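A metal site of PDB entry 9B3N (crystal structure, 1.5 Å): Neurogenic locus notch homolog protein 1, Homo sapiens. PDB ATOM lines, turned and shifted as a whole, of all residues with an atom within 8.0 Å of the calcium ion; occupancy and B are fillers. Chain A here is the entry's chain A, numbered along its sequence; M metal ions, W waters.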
ATOM      1  N   GLU A  29     -24.866  13.034  -2.144  1.00  0.00           N
ATOM      2  CA  GLU A  29     -26.069  12.941  -1.333  1.00  0.00           C
ATOM      3  C   GLU A  29     -26.269  14.220  -0.536  1.00  0.00           C
ATOM      4  O   GLU A  29     -25.329  14.723   0.088  1.00  0.00           O
ATOM      5  CB  GLU A  29     -25.963  11.736  -0.405  1.00  0.00           C
ATOM      6  CG  GLU A  29     -27.195  11.444   0.429  1.00  0.00           C
ATOM      7  CD  GLU A  29     -26.874  10.520   1.582  1.00  0.00           C
ATOM      8  OE1 GLU A  29     -25.756   9.952   1.574  1.00  0.00           O
ATOM      9  OE2 GLU A  29     -27.733  10.359   2.487  1.00  0.00           O
ATOM     10  N   GLY A  30     -27.481  14.741  -0.572  1.00  0.00           N
ATOM     11  CA  GLY A  30     -27.804  15.951   0.129  1.00  0.00           C
ATOM     12  C   GLY A  30     -27.827  17.199  -0.721  1.00  0.00           C
ATOM     13  O   GLY A  30     -28.309  18.240  -0.261  1.00  0.00           O
ATOM     14  N   PHE A  31     -27.355  17.123  -1.960  1.00  0.00           N
ATOM     15  CA  PHE A  31     -27.381  18.257  -2.888  1.00  0.00           C
ATOM     16  C   PHE A  31     -28.253  17.967  -4.103  1.00  0.00           C
ATOM     17  O   PHE A  31     -28.510  16.822  -4.471  1.00  0.00           O
ATOM     18  CB  PHE A  31     -25.943  18.654  -3.297  1.00  0.00           C
ATOM     19  CG  PHE A  31     -25.138  19.004  -2.105  1.00  0.00           C
ATOM     20  CD1 PHE A  31     -25.195  20.284  -1.600  1.00  0.00           C
ATOM     21  CD2 PHE A  31     -24.345  18.040  -1.483  1.00  0.00           C
ATOM     22  CE1 PHE A  31     -24.490  20.606  -0.414  1.00  0.00           C
ATOM     23  CE2 PHE A  31     -23.638  18.377  -0.294  1.00  0.00           C
ATOM     24  CZ  PHE A  31     -23.686  19.657   0.171  1.00  0.00           C
ATOM     25  N   THR A  38     -27.715  23.375  -4.603  1.00  0.00           N
ATOM     26  CA  THR A  38     -28.689  23.467  -3.536  1.00  0.00           C
ATOM     27  C   THR A  38     -28.403  22.427  -2.458  1.00  0.00           C
ATOM     28  O   THR A  38     -28.229  21.237  -2.731  1.00  0.00           O
ATOM     29  CB  THR A  38     -30.104  23.305  -4.075  1.00  0.00           C
ATOM     30  OG1 THR A  38     -30.401  24.402  -4.949  1.00  0.00           O
ATOM     31  CG2 THR A  38     -31.100  23.261  -2.916  1.00  0.00           C
ATOM     32  N   ASN A  39     -28.328  22.888  -1.225  1.00  0.00           N
ATOM     33  CA  ASN A  39     -28.248  21.980  -0.098  1.00  0.00           C
ATOM     34  C   ASN A  39     -29.703  21.683   0.268  1.00  0.00           C
ATOM     35  O   ASN A  39     -30.446  22.570   0.714  1.00  0.00           O
ATOM     36  CB  ASN A  39     -27.441  22.599   1.038  1.00  0.00           C
ATOM     37  CG  ASN A  39     -27.325  21.666   2.277  1.00  0.00           C
ATOM     38  OD1 ASN A  39     -28.223  20.829   2.537  1.00  0.00           O
ATOM     39  ND2 ASN A  39     -26.250  21.840   3.027  1.00  0.00           N
ATOM     40  N   ILE A  40     -30.137  20.449   0.024  1.00  0.00           N
ATOM     41  CA  ILE A  40     -31.519  20.085   0.279  1.00  0.00           C
ATOM     42  C   ILE A  40     -31.888  20.381   1.739  1.00  0.00           C
ATOM     43  O   ILE A  40     -31.107  20.121   2.661  1.00  0.00           O
ATOM     44  CB  ILE A  40     -31.756  18.597  -0.044  1.00  0.00           C
ATOM     45  CG1 ILE A  40     -31.531  18.329  -1.528  1.00  0.00           C
ATOM     46  CG2 ILE A  40     -33.178  18.153   0.301  1.00  0.00           C
ATOM     47  CD1 ILE A  40     -31.692  16.865  -1.946  1.00  0.00           C
ATOM     48  N   ASN A  41     -33.057  20.981   1.934  1.00  0.00           N
ATOM     49  CA  ASN A  41     -33.478  21.338   3.289  1.00  0.00           C
ATOM     50  C   ASN A  41     -34.253  20.153   3.867  1.00  0.00           C
ATOM     51  O   ASN A  41     -35.430  19.989   3.621  1.00  0.00           O
ATOM     52  CB  ASN A  41     -34.291  22.618   3.284  1.00  0.00           C
ATOM     53  CG  ASN A  41     -34.704  23.015   4.686  1.00  0.00           C
ATOM     54  OD1 ASN A  41     -34.111  22.560   5.691  1.00  0.00           O
ATOM     55  ND2 ASN A  41     -35.704  23.882   4.786  1.00  0.00           N
ATOM     56  N   GLU A  42     -33.577  19.296   4.617  1.00  0.00           N
ATOM     57  CA  GLU A  42     -34.268  18.144   5.216  1.00  0.00           C
ATOM     58  C   GLU A  42     -35.189  18.576   6.360  1.00  0.00           C
ATOM     59  O   GLU A  42     -36.033  17.770   6.804  1.00  0.00           O
ATOM     60  CB  GLU A  42     -33.262  17.082   5.705  1.00  0.00           C
ATOM     61  CG  GLU A  42     -32.649  16.205   4.535  1.00  0.00           C
ATOM     62  CD  GLU A  42     -31.454  16.842   3.886  1.00  0.00           C
ATOM     63  OE1 GLU A  42     -31.110  16.556   2.690  1.00  0.00           O
ATOM     64  OE2 GLU A  42     -30.816  17.656   4.546  1.00  0.00           O
ATOM     65  N   CYS A  43     -35.108  19.833   6.777  1.00  0.00           N
ATOM     66  CA  CYS A  43     -35.981  20.376   7.821  1.00  0.00           C
ATOM     67  C   CYS A  43     -37.343  20.772   7.276  1.00  0.00           C
ATOM     68  O   CYS A  43     -38.218  21.221   8.057  1.00  0.00           O
ATOM     69  CB  CYS A  43     -35.314  21.582   8.475  1.00  0.00           C
ATOM     70  SG  CYS A  43     -33.939  21.093   9.481  1.00  0.00           S
ATOM     71  N   ILE A  55     -32.284  21.935  12.590  1.00  0.00           N
ATOM     72  CA  ILE A  55     -31.032  22.476  12.065  1.00  0.00           C
ATOM     73  C   ILE A  55     -30.644  21.583  10.893  1.00  0.00           C
ATOM     74  O   ILE A  55     -30.509  20.362  11.040  1.00  0.00           O
ATOM     75  CB  ILE A  55     -29.930  22.488  13.152  1.00  0.00           C
ATOM     76  CG1 ILE A  55     -30.427  23.192  14.422  1.00  0.00           C
ATOM     77  CG2 ILE A  55     -28.619  23.076  12.575  1.00  0.00           C
ATOM     78  CD1 ILE A  55     -30.579  24.668  14.198  1.00  0.00           C
ATOM     79  N   ASP A  56     -30.546  22.177   9.707  1.00  0.00           N
ATOM     80  CA  ASP A  56     -30.302  21.367   8.527  1.00  0.00           C
ATOM     81  C   ASP A  56     -28.842  20.910   8.502  1.00  0.00           C
ATOM     82  O   ASP A  56     -27.952  21.574   9.033  1.00  0.00           O
ATOM     83  CB  ASP A  56     -30.662  22.177   7.286  1.00  0.00           C
ATOM     84  CG  ASP A  56     -30.363  21.450   5.997  1.00  0.00           C
ATOM     85  OD1 ASP A  56     -30.969  20.400   5.706  1.00  0.00           O
ATOM     86  OD2 ASP A  56     -29.459  21.921   5.279  1.00  0.00           O
ATOM     87  N   ASP A  57     -28.637  19.707   7.978  1.00  0.00           N
ATOM     88  CA  ASP A  57     -27.305  19.161   7.785  1.00  0.00           C
ATOM     89  C   ASP A  57     -27.157  18.738   6.329  1.00  0.00           C
ATOM     90  O   ASP A  57     -28.079  18.861   5.522  1.00  0.00           O
ATOM     91  CB  ASP A  57     -27.069  17.964   8.720  1.00  0.00           C
ATOM     92  CG  ASP A  57     -25.575  17.719   9.058  1.00  0.00           C
ATOM     93  OD1 ASP A  57     -24.639  18.162   8.345  1.00  0.00           O
ATOM     94  OD2 ASP A  57     -25.349  17.020  10.097  1.00  0.00           O
ATOM     95  N   VAL A  58     -25.991  18.193   5.990  1.00  0.00           N
ATOM     96  CA  VAL A  58     -25.836  17.540   4.698  1.00  0.00           C
ATOM     97  C   VAL A  58     -26.484  16.152   4.794  1.00  0.00           C
ATOM     98  O   VAL A  58     -26.047  15.301   5.585  1.00  0.00           O
ATOM     99  CB  VAL A  58     -24.380  17.457   4.295  1.00  0.00           C
ATOM    100  CG1 VAL A  58     -24.266  16.638   2.985  1.00  0.00           C
ATOM    101  CG2 VAL A  58     -23.859  18.857   4.104  1.00  0.00           C
ATOM    102  N   ALA A  59     -27.614  15.989   4.096  1.00  0.00           N
ATOM    103  CA  ALA A  59     -28.336  14.713   4.040  1.00  0.00           C
ATOM    104  C   ALA A  59     -28.840  14.330   5.415  1.00  0.00           C
ATOM    105  O   ALA A  59     -28.733  13.183   5.836  1.00  0.00           O
ATOM    106  CB  ALA A  59     -27.479  13.583   3.489  1.00  0.00           C
ATOM    107  N   GLY A  60     -29.342  15.314   6.141  1.00  0.00           N
ATOM    108  CA  GLY A  60     -29.840  15.026   7.480  1.00  0.00           C
ATOM    109  C   GLY A  60     -30.165  16.301   8.192  1.00  0.00           C
ATOM    110  O   GLY A  60     -30.110  17.402   7.637  1.00  0.00           O
ATOM    111  N   TYR A  61     -30.611  16.120   9.444  1.00  0.00           N
ATOM    112  CA  TYR A  61     -30.966  17.252  10.257  1.00  0.00           C
ATOM    113  C   TYR A  61     -30.727  16.846  11.703  1.00  0.00           C
ATOM    114  O   TYR A  61     -30.551  15.660  12.023  1.00  0.00           O
ATOM    115  CB  TYR A  61     -32.440  17.658  10.034  1.00  0.00           C
ATOM    116  CG  TYR A  61     -33.382  16.607  10.618  1.00  0.00           C
ATOM    117  CD1 TYR A  61     -33.818  16.690  11.963  1.00  0.00           C
ATOM    118  CD2 TYR A  61     -33.790  15.501   9.863  1.00  0.00           C
ATOM    119  CE1 TYR A  61     -34.606  15.710  12.517  1.00  0.00           C
ATOM    120  CE2 TYR A  61     -34.624  14.516  10.439  1.00  0.00           C
ATOM    121  CZ  TYR A  61     -35.022  14.635  11.759  1.00  0.00           C
ATOM    122  OH  TYR A  61     -35.830  13.682  12.342  1.00  0.00           O
HETATM  123 CA    CA M   1     -29.534  19.682   4.019  1.00  0.00          CA
HETATM  124  O   HOH W   1     -28.806  17.931   2.453  1.00  0.00           O
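The nearest printed residue that does not touch the calcium ion is Ala 59 (4.2 Å).
The side-chain sulfur of Cys 43 lies within hydrogen-bond range of the backbone NH of Asp 56 (3.6 Å).
The side-chain carboxylate (OE2) of Glu 42 lies close to the backbone NH (N) of Gly 60.
N of Ile 40 lies within hydrogen-bond range of O of Gly 30.
The calcium ion is bound by the backbone carbonyl oxygen (O) of Ile 40 (2.1 Å), the backbone carbonyl oxygen (O) of Asp 57 (2.2 Å), the side-chain amide oxygen (OD1) of Asn 39 (2.3 Å), the side-chain carboxylate (OD1) of Asp 56 (2.3 Å), the side-chain carboxylate (OE2) of Glu 42 (2.5 Å), water W1 (2.5 Å) and the side-chain carboxylate (OD2) of Asp 56 (2.6 Å).
Water W1 lies within hydrogen-bond range of OE1 of Glu 42, O of Gly 30 and N of Ala 59.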
